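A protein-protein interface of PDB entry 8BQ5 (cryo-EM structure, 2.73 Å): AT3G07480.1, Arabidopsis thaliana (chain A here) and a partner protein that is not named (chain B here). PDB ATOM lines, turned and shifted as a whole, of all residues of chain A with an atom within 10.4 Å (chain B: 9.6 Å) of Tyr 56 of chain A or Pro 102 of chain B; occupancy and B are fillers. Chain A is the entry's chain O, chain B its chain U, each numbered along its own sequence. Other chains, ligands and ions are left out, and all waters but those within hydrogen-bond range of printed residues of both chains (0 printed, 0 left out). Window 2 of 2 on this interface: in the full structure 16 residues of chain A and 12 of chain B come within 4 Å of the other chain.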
ATOM      1  N   LEU A  48      35.770  18.224 -25.533  1.00  0.00           N
ATOM      2  CA  LEU A  48      34.419  17.924 -25.085  1.00  0.00           C
ATOM      3  C   LEU A  48      34.143  18.633 -23.772  1.00  0.00           C
ATOM      4  O   LEU A  48      35.063  19.054 -23.067  1.00  0.00           O
ATOM      5  CB  LEU A  48      34.192  16.422 -24.877  1.00  0.00           C
ATOM      6  CG  LEU A  48      34.189  15.493 -26.084  1.00  0.00           C
ATOM      7  CD1 LEU A  48      34.356  14.056 -25.633  1.00  0.00           C
ATOM      8  CD2 LEU A  48      32.905  15.673 -26.851  1.00  0.00           C
ATOM      9  N   SER A  49      32.862  18.748 -23.444  1.00  0.00           N
ATOM     10  CA  SER A  49      32.430  19.215 -22.137  1.00  0.00           C
ATOM     11  C   SER A  49      31.369  18.264 -21.606  1.00  0.00           C
ATOM     12  O   SER A  49      30.542  17.758 -22.368  1.00  0.00           O
ATOM     13  CB  SER A  49      31.876  20.633 -22.204  1.00  0.00           C
ATOM     14  OG  SER A  49      32.890  21.546 -22.569  1.00  0.00           O
ATOM     15  N   ALA A  50      31.399  18.020 -20.301  1.00  0.00           N
ATOM     16  CA  ALA A  50      30.444  17.131 -19.659  1.00  0.00           C
ATOM     17  C   ALA A  50      29.856  17.809 -18.433  1.00  0.00           C
ATOM     18  O   ALA A  50      30.586  18.387 -17.623  1.00  0.00           O
ATOM     19  CB  ALA A  50      31.097  15.805 -19.262  1.00  0.00           C
ATOM     20  N   ILE A  51      28.535  17.738 -18.304  1.00  0.00           N
ATOM     21  CA  ILE A  51      27.821  18.296 -17.160  1.00  0.00           C
ATOM     22  C   ILE A  51      27.443  17.148 -16.235  1.00  0.00           C
ATOM     23  O   ILE A  51      26.692  16.245 -16.624  1.00  0.00           O
ATOM     24  CB  ILE A  51      26.585  19.094 -17.603  1.00  0.00           C
ATOM     25  CG1 ILE A  51      27.010  20.368 -18.334  1.00  0.00           C
ATOM     26  CG2 ILE A  51      25.703  19.426 -16.416  1.00  0.00           C
ATOM     27  CD1 ILE A  51      25.919  20.976 -19.179  1.00  0.00           C
ATOM     28  N   ASP A  52      27.961  17.189 -15.010  1.00  0.00           N
ATOM     29  CA  ASP A  52      27.788  16.106 -14.057  1.00  0.00           C
ATOM     30  C   ASP A  52      26.399  16.167 -13.413  1.00  0.00           C
ATOM     31  O   ASP A  52      25.671  17.146 -13.588  1.00  0.00           O
ATOM     32  CB  ASP A  52      28.911  16.166 -13.014  1.00  0.00           C
ATOM     33  CG  ASP A  52      28.865  17.423 -12.156  1.00  0.00           C
ATOM     34  OD1 ASP A  52      29.919  17.811 -11.614  1.00  0.00           O
ATOM     35  OD2 ASP A  52      27.790  18.035 -12.019  1.00  0.00           O
ATOM     36  N   PRO A  53      26.004  15.125 -12.669  1.00  0.00           N
ATOM     37  CA  PRO A  53      24.681  15.160 -12.020  1.00  0.00           C
ATOM     38  C   PRO A  53      24.469  16.358 -11.116  1.00  0.00           C
ATOM     39  O   PRO A  53      23.336  16.843 -11.002  1.00  0.00           O
ATOM     40  CB  PRO A  53      24.658  13.852 -11.222  1.00  0.00           C
ATOM     41  CG  PRO A  53      25.503  12.946 -12.005  1.00  0.00           C
ATOM     42  CD  PRO A  53      26.624  13.795 -12.535  1.00  0.00           C
ATOM     43  N   ASP A  54      25.516  16.849 -10.457  1.00  0.00           N
ATOM     44  CA  ASP A  54      25.356  18.021  -9.609  1.00  0.00           C
ATOM     45  C   ASP A  54      25.351  19.329 -10.396  1.00  0.00           C
ATOM     46  O   ASP A  54      25.182  20.392  -9.790  1.00  0.00           O
ATOM     47  CB  ASP A  54      26.408  17.978  -8.475  1.00  0.00           C
ATOM     48  CG  ASP A  54      26.138  16.926  -7.457  1.00  0.00           C
ATOM     49  OD1 ASP A  54      25.062  16.338  -7.339  1.00  0.00           O
ATOM     50  OD2 ASP A  54      27.056  16.567  -6.807  1.00  0.00           O
ATOM     51  N   GLY A  55      25.555  19.280 -11.711  1.00  0.00           N
ATOM     52  CA  GLY A  55      25.368  20.430 -12.568  1.00  0.00           C
ATOM     53  C   GLY A  55      26.629  21.164 -12.970  1.00  0.00           C
ATOM     54  O   GLY A  55      26.548  22.092 -13.783  1.00  0.00           O
ATOM     55  N   TYR A  56      27.784  20.787 -12.436  1.00  0.00           N
ATOM     56  CA  TYR A  56      29.014  21.502 -12.746  1.00  0.00           C
ATOM     57  C   TYR A  56      29.656  20.956 -14.015  1.00  0.00           C
ATOM     58  O   TYR A  56      29.745  19.743 -14.221  1.00  0.00           O
ATOM     59  CB  TYR A  56      29.992  21.448 -11.570  1.00  0.00           C
ATOM     60  CG  TYR A  56      29.554  22.156 -10.283  1.00  0.00           C
ATOM     61  CD1 TYR A  56      29.792  23.479 -10.072  1.00  0.00           C
ATOM     62  CD2 TYR A  56      28.791  21.523  -9.357  1.00  0.00           C
ATOM     63  CE1 TYR A  56      29.372  24.081  -8.892  1.00  0.00           C
ATOM     64  CE2 TYR A  56      28.432  22.069  -8.168  1.00  0.00           C
ATOM     65  CZ  TYR A  56      28.687  23.358  -7.941  1.00  0.00           C
ATOM     66  OH  TYR A  56      28.257  23.938  -6.775  1.00  0.00           O
ATOM     67  N   LYS A  57      30.096  21.877 -14.867  1.00  0.00           N
ATOM     68  CA  LYS A  57      30.567  21.564 -16.208  1.00  0.00           C
ATOM     69  C   LYS A  57      32.070  21.328 -16.200  1.00  0.00           C
ATOM     70  O   LYS A  57      32.823  22.063 -15.554  1.00  0.00           O
ATOM     71  CB  LYS A  57      30.212  22.709 -17.156  1.00  0.00           C
ATOM     72  CG  LYS A  57      30.426  22.444 -18.632  1.00  0.00           C
ATOM     73  CD  LYS A  57      29.695  23.503 -19.444  1.00  0.00           C
ATOM     74  CE  LYS A  57      29.964  23.378 -20.929  1.00  0.00           C
ATOM     75  NZ  LYS A  57      28.908  24.064 -21.721  1.00  0.00           N
ATOM     76  N   GLN A  58      32.504  20.294 -16.917  1.00  0.00           N
ATOM     77  CA  GLN A  58      33.905  19.903 -16.963  1.00  0.00           C
ATOM     78  C   GLN A  58      34.346  19.720 -18.405  1.00  0.00           C
ATOM     79  O   GLN A  58      33.623  19.137 -19.215  1.00  0.00           O
ATOM     80  CB  GLN A  58      34.152  18.603 -16.195  1.00  0.00           C
ATOM     81  CG  GLN A  58      34.419  18.795 -14.719  1.00  0.00           C
ATOM     82  CD  GLN A  58      33.204  18.480 -13.877  1.00  0.00           C
ATOM     83  OE1 GLN A  58      32.437  17.571 -14.194  1.00  0.00           O
ATOM     84  NE2 GLN A  58      33.018  19.233 -12.801  1.00  0.00           N
ATOM     85  N   ASP A  59      35.542  20.206 -18.713  1.00  0.00           N
ATOM     86  CA  ASP A  59      36.123  20.032 -20.036  1.00  0.00           C
ATOM     87  C   ASP A  59      36.924  18.737 -20.055  1.00  0.00           C
ATOM     88  O   ASP A  59      37.907  18.597 -19.319  1.00  0.00           O
ATOM     89  CB  ASP A  59      36.997  21.229 -20.399  1.00  0.00           C
ATOM     90  CG  ASP A  59      36.210  22.322 -21.086  1.00  0.00           C
ATOM     91  OD1 ASP A  59      36.490  23.512 -20.835  1.00  0.00           O
ATOM     92  OD2 ASP A  59      35.299  21.987 -21.871  1.00  0.00           O
ATOM     93  N   ILE A  60      36.498  17.790 -20.886  1.00  0.00           N
ATOM     94  CA  ILE A  60      37.101  16.468 -20.942  1.00  0.00           C
ATOM     95  C   ILE A  60      37.676  16.240 -22.334  1.00  0.00           C
ATOM     96  O   ILE A  60      37.404  16.982 -23.278  1.00  0.00           O
ATOM     97  CB  ILE A  60      36.107  15.352 -20.572  1.00  0.00           C
ATOM     98  CG1 ILE A  60      35.154  15.093 -21.734  1.00  0.00           C
ATOM     99  CG2 ILE A  60      35.348  15.714 -19.309  1.00  0.00           C
ATOM    100  CD1 ILE A  60      34.063  14.123 -21.415  1.00  0.00           C
ATOM    101  N   LEU A  72      34.739   9.584 -21.236  1.00  0.00           N
ATOM    102  CA  LEU A  72      34.114   9.841 -19.944  1.00  0.00           C
ATOM    103  C   LEU A  72      34.805   9.080 -18.818  1.00  0.00           C
ATOM    104  O   LEU A  72      34.823   9.548 -17.676  1.00  0.00           O
ATOM    105  CB  LEU A  72      32.634   9.476 -20.013  1.00  0.00           C
ATOM    106  CG  LEU A  72      31.801  10.411 -20.892  1.00  0.00           C
ATOM    107  CD1 LEU A  72      30.422   9.842 -21.148  1.00  0.00           C
ATOM    108  CD2 LEU A  72      31.704  11.776 -20.253  1.00  0.00           C
ATOM    109  N   LEU A  77      34.487  10.249 -14.825  1.00  0.00           N
ATOM    110  CA  LEU A  77      33.112  10.734 -14.849  1.00  0.00           C
ATOM    111  C   LEU A  77      32.131   9.572 -14.863  1.00  0.00           C
ATOM    112  O   LEU A  77      31.093   9.612 -14.194  1.00  0.00           O
ATOM    113  CB  LEU A  77      32.893  11.644 -16.054  1.00  0.00           C
ATOM    114  CG  LEU A  77      33.367  13.077 -15.818  1.00  0.00           C
ATOM    115  CD1 LEU A  77      33.135  13.927 -17.045  1.00  0.00           C
ATOM    116  CD2 LEU A  77      32.661  13.669 -14.614  1.00  0.00           C
ATOM    117  N   VAL A 147      28.549  19.317 -25.909  1.00  0.00           N
ATOM    118  CA  VAL A 147      28.218  19.245 -24.491  1.00  0.00           C
ATOM    119  C   VAL A 147      27.407  17.982 -24.247  1.00  0.00           C
ATOM    120  O   VAL A 147      26.465  17.682 -24.991  1.00  0.00           O
ATOM    121  CB  VAL A 147      27.443  20.489 -24.029  1.00  0.00           C
ATOM    122  CG1 VAL A 147      27.343  20.509 -22.512  1.00  0.00           C
ATOM    123  CG2 VAL A 147      28.113  21.750 -24.540  1.00  0.00           C
ATOM    124  N   VAL A 148      27.774  17.241 -23.208  1.00  0.00           N
ATOM    125  CA  VAL A 148      27.116  15.996 -22.841  1.00  0.00           C
ATOM    126  C   VAL A 148      26.715  16.082 -21.376  1.00  0.00           C
ATOM    127  O   VAL A 148      27.462  16.617 -20.552  1.00  0.00           O
ATOM    128  CB  VAL A 148      28.037  14.784 -23.101  1.00  0.00           C
ATOM    129  CG1 VAL A 148      27.693  13.622 -22.187  1.00  0.00           C
ATOM    130  CG2 VAL A 148      27.944  14.366 -24.553  1.00  0.00           C
ATOM    131  N   ALA A 149      25.525  15.584 -21.054  1.00  0.00           N
ATOM    132  CA  ALA A 149      25.040  15.551 -19.681  1.00  0.00           C
ATOM    133  C   ALA A 149      25.159  14.137 -19.126  1.00  0.00           C
ATOM    134  O   ALA A 149      24.639  13.187 -19.717  1.00  0.00           O
ATOM    135  CB  ALA A 149      23.593  16.033 -19.603  1.00  0.00           C
ATOM    136  N   VAL A 150      25.831  14.004 -17.986  1.00  0.00           N
ATOM    137  CA  VAL A 150      26.074  12.706 -17.362  1.00  0.00           C
ATOM    138  C   VAL A 150      25.018  12.504 -16.278  1.00  0.00           C
ATOM    139  O   VAL A 150      25.046  13.215 -15.261  1.00  0.00           O
ATOM    140  CB  VAL A 150      27.490  12.620 -16.780  1.00  0.00           C
ATOM    141  CG1 VAL A 150      27.662  11.333 -15.984  1.00  0.00           C
ATOM    142  CG2 VAL A 150      28.519  12.714 -17.889  1.00  0.00           C
ATOM    143  N   PRO A 151      24.093  11.563 -16.438  1.00  0.00           N
ATOM    144  CA  PRO A 151      23.075  11.336 -15.410  1.00  0.00           C
ATOM    145  C   PRO A 151      23.650  10.579 -14.220  1.00  0.00           C
ATOM    146  O   PRO A 151      24.778  10.087 -14.241  1.00  0.00           O
ATOM    147  CB  PRO A 151      22.020  10.501 -16.140  1.00  0.00           C
ATOM    148  CG  PRO A 151      22.790   9.761 -17.167  1.00  0.00           C
ATOM    149  CD  PRO A 151      23.930  10.658 -17.587  1.00  0.00           C
ATOM    150  N   VAL B  90      22.108  37.808 -15.367  1.00  0.00           N
ATOM    151  CA  VAL B  90      22.442  36.392 -15.288  1.00  0.00           C
ATOM    152  C   VAL B  90      21.581  35.692 -14.247  1.00  0.00           C
ATOM    153  O   VAL B  90      21.080  34.586 -14.480  1.00  0.00           O
ATOM    154  CB  VAL B  90      23.942  36.207 -15.009  1.00  0.00           C
ATOM    155  CG1 VAL B  90      24.275  34.734 -14.949  1.00  0.00           C
ATOM    156  CG2 VAL B  90      24.745  36.870 -16.106  1.00  0.00           C
ATOM    157  N   MET B  91      21.375  36.317 -13.091  1.00  0.00           N
ATOM    158  CA  MET B  91      20.531  35.643 -12.116  1.00  0.00           C
ATOM    159  C   MET B  91      19.051  35.753 -12.486  1.00  0.00           C
ATOM    160  O   MET B  91      18.251  34.921 -12.045  1.00  0.00           O
ATOM    161  CB  MET B  91      20.798  36.176 -10.711  1.00  0.00           C
ATOM    162  CG  MET B  91      20.892  35.053  -9.671  1.00  0.00           C
ATOM    163  SD  MET B  91      20.359  35.500  -8.037  1.00  0.00           S
ATOM    164  CE  MET B  91      18.586  35.267  -8.242  1.00  0.00           C
ATOM    165  N   GLU B  94      18.543  32.740 -13.977  1.00  0.00           N
ATOM    166  CA  GLU B  94      18.427  31.661 -13.002  1.00  0.00           C
ATOM    167  C   GLU B  94      16.998  31.513 -12.499  1.00  0.00           C
ATOM    168  O   GLU B  94      16.526  30.395 -12.267  1.00  0.00           O
ATOM    169  CB  GLU B  94      19.380  31.889 -11.827  1.00  0.00           C
ATOM    170  CG  GLU B  94      20.841  31.620 -12.133  1.00  0.00           C
ATOM    171  CD  GLU B  94      21.774  32.216 -11.097  1.00  0.00           C
ATOM    172  OE1 GLU B  94      21.690  31.814  -9.916  1.00  0.00           O
ATOM    173  OE2 GLU B  94      22.598  33.079 -11.462  1.00  0.00           O
ATOM    174  N   PHE B  99      17.233  27.214 -12.073  1.00  0.00           N
ATOM    175  CA  PHE B  99      18.432  26.485 -11.687  1.00  0.00           C
ATOM    176  C   PHE B  99      19.562  27.478 -11.473  1.00  0.00           C
ATOM    177  O   PHE B  99      19.536  28.600 -11.984  1.00  0.00           O
ATOM    178  CB  PHE B  99      18.796  25.412 -12.724  1.00  0.00           C
ATOM    179  CG  PHE B  99      19.717  25.891 -13.809  1.00  0.00           C
ATOM    180  CD1 PHE B  99      21.088  25.734 -13.700  1.00  0.00           C
ATOM    181  CD2 PHE B  99      19.205  26.477 -14.952  1.00  0.00           C
ATOM    182  CE1 PHE B  99      21.929  26.169 -14.702  1.00  0.00           C
ATOM    183  CE2 PHE B  99      20.041  26.911 -15.958  1.00  0.00           C
ATOM    184  CZ  PHE B  99      21.403  26.756 -15.834  1.00  0.00           C
ATOM    185  N   GLU B 100      20.557  27.054 -10.700  1.00  0.00           N
ATOM    186  CA  GLU B 100      21.653  27.926 -10.306  1.00  0.00           C
ATOM    187  C   GLU B 100      22.835  27.726 -11.243  1.00  0.00           C
ATOM    188  O   GLU B 100      23.282  26.595 -11.459  1.00  0.00           O
ATOM    189  CB  GLU B 100      22.071  27.651  -8.862  1.00  0.00           C
ATOM    190  CG  GLU B 100      20.932  27.731  -7.857  1.00  0.00           C
ATOM    191  CD  GLU B 100      20.316  29.112  -7.786  1.00  0.00           C
ATOM    192  OE1 GLU B 100      21.066  30.084  -7.583  1.00  0.00           O
ATOM    193  OE2 GLU B 100      19.082  29.228  -7.934  1.00  0.00           O
ATOM    194  N   ILE B 101      23.335  28.821 -11.793  1.00  0.00           N
ATOM    195  CA  ILE B 101      24.474  28.803 -12.708  1.00  0.00           C
ATOM    196  C   ILE B 101      25.748  28.926 -11.881  1.00  0.00           C
ATOM    197  O   ILE B 101      25.888  29.903 -11.131  1.00  0.00           O
ATOM    198  CB  ILE B 101      24.381  29.935 -13.745  1.00  0.00           C
ATOM    199  CG1 ILE B 101      23.093  29.801 -14.557  1.00  0.00           C
ATOM    200  CG2 ILE B 101      25.604  29.927 -14.647  1.00  0.00           C
ATOM    201  CD1 ILE B 101      22.987  30.780 -15.699  1.00  0.00           C
ATOM    202  N   PRO B 102      26.693  27.942 -11.931  1.00  0.00           N
ATOM    203  CA  PRO B 102      27.994  28.104 -11.273  1.00  0.00           C
ATOM    204  C   PRO B 102      28.595  29.448 -11.696  1.00  0.00           C
ATOM    205  O   PRO B 102      28.474  29.778 -12.856  1.00  0.00           O
ATOM    206  CB  PRO B 102      28.809  26.947 -11.848  1.00  0.00           C
ATOM    207  CG  PRO B 102      27.796  25.854 -12.025  1.00  0.00           C
ATOM    208  CD  PRO B 102      26.589  26.597 -12.545  1.00  0.00           C
ATOM    209  N   ASP B 103      29.241  30.172 -10.777  1.00  0.00           N
ATOM    210  CA  ASP B 103      29.733  31.548 -11.077  1.00  0.00           C
ATOM    211  C   ASP B 103      30.655  31.605 -12.299  1.00  0.00           C
ATOM    212  O   ASP B 103      30.502  32.537 -13.097  1.00  0.00           O
ATOM    213  CB  ASP B 103      30.437  32.157  -9.865  1.00  0.00           C
ATOM    214  CG  ASP B 103      29.491  32.449  -8.710  1.00  0.00           C
ATOM    215  OD1 ASP B 103      28.271  32.246  -8.883  1.00  0.00           O
ATOM    216  OD2 ASP B 103      29.982  32.875  -7.645  1.00  0.00           O
ATOM    217  N   ASN B 104      31.598  30.679 -12.423  1.00  0.00           N
ATOM    218  CA  ASN B 104      32.580  30.717 -13.538  1.00  0.00           C
ATOM    219  C   ASN B 104      31.831  30.589 -14.871  1.00  0.00           C
ATOM    220  O   ASN B 104      32.431  30.909 -15.915  1.00  0.00           O
ATOM    221  CB  ASN B 104      33.652  29.653 -13.336  1.00  0.00           C
ATOM    222  CG  ASN B 104      34.421  29.808 -12.040  1.00  0.00           C
ATOM    223  OD1 ASN B 104      34.138  30.699 -11.239  1.00  0.00           O
ATOM    224  ND2 ASN B 104      35.398  28.943 -11.824  1.00  0.00           N
ATOM    225  N   GLU B 105      30.591  30.099 -14.842  1.00  0.00           N
ATOM    226  CA  GLU B 105      29.755  30.054 -16.062  1.00  0.00           C
ATOM    227  C   GLU B 105      28.997  31.380 -16.122  1.00  0.00           C
ATOM    228  O   GLU B 105      28.875  31.938 -17.211  1.00  0.00           O
ATOM    229  CB  GLU B 105      28.821  28.848 -15.995  1.00  0.00           C
ATOM    230  CG  GLU B 105      29.541  27.558 -15.669  1.00  0.00           C
ATOM    231  CD  GLU B 105      30.684  27.255 -16.619  1.00  0.00           C
ATOM    232  OE1 GLU B 105      31.848  27.380 -16.192  1.00  0.00           O
ATOM    233  OE2 GLU B 105      30.404  26.897 -17.781  1.00  0.00           O
ATOM    234  N   ALA B 106      28.568  31.886 -14.967  1.00  0.00           N
ATOM    235  CA  ALA B 106      27.848  33.179 -14.904  1.00  0.00           C
ATOM    236  C   ALA B 106      28.708  34.285 -15.524  1.00  0.00           C
ATOM    237  O   ALA B 106      28.132  35.313 -15.913  1.00  0.00           O
ATOM    238  CB  ALA B 106      27.509  33.490 -13.473  1.00  0.00           C
ATOM    239  N   ASP B 107      30.026  34.070 -15.609  1.00  0.00           N
ATOM    240  CA  ASP B 107      30.953  35.093 -16.161  1.00  0.00           C
ATOM    241  C   ASP B 107      31.152  34.894 -17.665  1.00  0.00           C
ATOM    242  O   ASP B 107      31.263  35.904 -18.376  1.00  0.00           O
ATOM    243  CB  ASP B 107      32.289  35.088 -15.413  1.00  0.00           C
ATOM    244  CG  ASP B 107      32.127  35.144 -13.903  1.00  0.00           C
ATOM    245  OD1 ASP B 107      31.179  35.806 -13.440  1.00  0.00           O
ATOM    246  OD2 ASP B 107      32.939  34.505 -13.204  1.00  0.00           O
ATOM    247  N   LYS B 108      31.173  33.645 -18.139  1.00  0.00           N
ATOM    248  CA  LYS B 108      31.280  33.428 -19.604  1.00  0.00           C
ATOM    249  C   LYS B 108      29.906  33.661 -20.252  1.00  0.00           C
ATOM    250  O   LYS B 108      29.726  33.213 -21.389  1.00  0.00           O
ATOM    251  CB  LYS B 108      31.903  32.056 -19.896  1.00  0.00           C
ATOM    252  CG  LYS B 108      31.124  30.844 -19.406  1.00  0.00           C
ATOM    253  CD  LYS B 108      31.750  29.533 -19.828  1.00  0.00           C
ATOM    254  CE  LYS B 108      33.218  29.428 -19.470  1.00  0.00           C
ATOM    255  NZ  LYS B 108      33.436  29.503 -18.007  1.00  0.00           N
ATOM    256  N   ILE B 109      28.968  34.315 -19.550  1.00  0.00           N
ATOM    257  CA  ILE B 109      27.650  34.676 -20.154  1.00  0.00           C
ATOM    258  C   ILE B 109      27.671  36.201 -20.285  1.00  0.00           C
ATOM    259  O   ILE B 109      27.125  36.905 -19.409  1.00  0.00           O
ATOM    260  CB  ILE B 109      26.464  34.144 -19.321  1.00  0.00           C
ATOM    261  CG1 ILE B 109      26.394  32.616 -19.347  1.00  0.00           C
ATOM    262  CG2 ILE B 109      25.147  34.759 -19.760  1.00  0.00           C
ATOM    263  CD1 ILE B 109      25.203  32.050 -18.611  1.00  0.00           C
ATOM    264  N   PHE B 118      24.415  28.150 -23.153  1.00  0.00           N
ATOM    265  CA  PHE B 118      24.579  27.486 -21.867  1.00  0.00           C
ATOM    266  C   PHE B 118      23.278  26.848 -21.393  1.00  0.00           C
ATOM    267  O   PHE B 118      23.264  25.694 -20.952  1.00  0.00           O
ATOM    268  CB  PHE B 118      25.102  28.482 -20.835  1.00  0.00           C
ATOM    269  CG  PHE B 118      25.340  27.875 -19.494  1.00  0.00           C
ATOM    270  CD1 PHE B 118      26.306  26.899 -19.329  1.00  0.00           C
ATOM    271  CD2 PHE B 118      24.594  28.268 -18.399  1.00  0.00           C
ATOM    272  CE1 PHE B 118      26.522  26.325 -18.095  1.00  0.00           C
ATOM    273  CE2 PHE B 118      24.809  27.702 -17.165  1.00  0.00           C
ATOM    274  CZ  PHE B 118      25.776  26.731 -17.010  1.00  0.00           C
ATOM    275  N   HIS B 122      22.155  22.810 -20.728  1.00  0.00           N
ATOM    276  CA  HIS B 122      22.166  22.435 -19.318  1.00  0.00           C
ATOM    277  C   HIS B 122      20.937  21.597 -18.987  1.00  0.00           C
ATOM    278  O   HIS B 122      19.811  22.060 -19.198  1.00  0.00           O
ATOM    279  CB  HIS B 122      22.209  23.671 -18.431  1.00  0.00           C
ATOM    280  CG  HIS B 122      22.924  23.453 -17.135  1.00  0.00           C
ATOM    281  ND1 HIS B 122      22.305  22.921 -16.024  1.00  0.00           N
ATOM    282  CD2 HIS B 122      24.210  23.679 -16.777  1.00  0.00           C
ATOM    283  CE1 HIS B 122      23.175  22.837 -15.036  1.00  0.00           C
ATOM    284  NE2 HIS B 122      24.339  23.290 -15.465  1.00  0.00           N
ATOM    285  N   PRO B 123      21.103  20.371 -18.484  1.00  0.00           N
ATOM    286  CA  PRO B 123      19.927  19.552 -18.145  1.00  0.00           C
ATOM    287  C   PRO B 123      19.072  20.120 -17.023  1.00  0.00           C
ATOM    288  O   PRO B 123      17.854  19.905 -17.020  1.00  0.00           O
ATOM    289  CB  PRO B 123      20.549  18.204 -17.757  1.00  0.00           C
ATOM    290  CG  PRO B 123      21.918  18.549 -17.291  1.00  0.00           C
ATOM    291  CD  PRO B 123      22.366  19.685 -18.165  1.00  0.00           C
ATOM    292  N   GLN B 124      19.663  20.839 -16.066  1.00  0.00           N
ATOM    293  CA  GLN B 124      18.893  21.353 -14.938  1.00  0.00           C
ATOM    294  C   GLN B 124      17.924  22.459 -15.338  1.00  0.00           C
ATOM    295  O   GLN B 124      17.088  22.853 -14.518  1.00  0.00           O
ATOM    296  CB  GLN B 124      19.838  21.852 -13.841  1.00  0.00           C
ATOM    297  CG  GLN B 124      20.526  20.737 -13.059  1.00  0.00           C
ATOM    298  CD  GLN B 124      21.486  21.264 -12.006  1.00  0.00           C
ATOM    299  OE1 GLN B 124      22.009  22.370 -12.126  1.00  0.00           O
ATOM    300  NE2 GLN B 124      21.723  20.468 -10.970  1.00  0.00           N
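Among the printed residues, merely in contact across the chains: Ile 51 of chain A with His 122 of chain B (3.9996 Å), Ile 51 of chain A with Pro 123 of chain B (3.8 Å), Pro 53 of chain A with Gln 124 of chain B (3.97 Å), Asp 54 of chain A with Gln 124 of chain B (3.7 Å), Gly 55 of chain A with Gln 124 of chain B (3.9 Å), Tyr 56 of chain A with Pro 102 of chain B (3.7 Å), Lys 57 of chain A with Glu 105 of chain B (3.8 Å) and Ala 149 of chain A with Pro 123 of chain B (3.8 Å).
N of Val 150 of chain A lies within hydrogen-bond range of O of Ile 51 of chain A (2.8 Å).
N of Asp 54 of chain A is in hydrogen-bond range of OD2 of Asp 52 of chain A (3.0 Å).
The side-chain carboxylate (OD2) of Asp 52 of chain A lies within hydrogen-bond range of the backbone NH (N) of Gly 55 of chain A (2.6 Å).
N of Tyr 56 of chain A sits at hydrogen-bond distance from OD2 of Asp 52 of chain A.
The backbone carbonyl oxygen (O) of Tyr 56 of chain A lies close to the side-chain amide oxygen (OE1) of Gln 58 of chain A.
N of Gln 124 of chain B sits close to ND1 of His 122 of chain B, at 3.4 Å.
O of Gly 55 of chain A sits at hydrogen-bond distance from NE2 of His 122 of chain B, 3.0 Å away.
Printed residues of chain A that touch a printed residue of chain B: Ile 51, Pro 53, Asp 54, Gly 55, Tyr 56, Lys 57 and Ala 149.
Hydrophobic or aromatic side chains of chain A within 4 Å of the printed part of chain B: Ile 51, Tyr 56 and Ala 149.
Of the 18 printed residues of chain B, 5 touch a printed residue of chain A.
Hydrophobic or aromatic side chains of chain B that line the printed part of chain A: Pro 102, His 122 and Pro 123.
Among the printed residues, no Asp or Glu carboxylate lies within 4 Å of a Lys or Arg side-chain nitrogen of the other chain.
Pro 102 of chain B touches one residue of chain A.
No residue of chain B comes within 4 Å of Asp 52 of chain A.
Of chain B, only His 122 and Gln 124 come within 4 Å of Gly 55 of chain A.
No residue of chain A comes within 4 Å of Asp 103 of chain B.
Glu 105 of chain B touches one residue of chain A.
No residue of chain A comes within 4 Å of Ala 106 of chain B.
Printed residues of chain B within 4 Å of Lys 57 of chain A: Glu 105 (3.8 Å).
Printed residues of chain B within 4 Å of Asp 54 of chain A: Gln 124.
Of the printed residues of chain A, Pro 123 of chain B touches Ile 51 (3.8 Å) and Ala 149 (3.8 Å).
Pro 151 of chain A touches none of the printed residues of chain B.
The nearest printed residue of chain A that does not touch Pro 123 of chain B is Asp 52 of chain A (5.5 Å).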
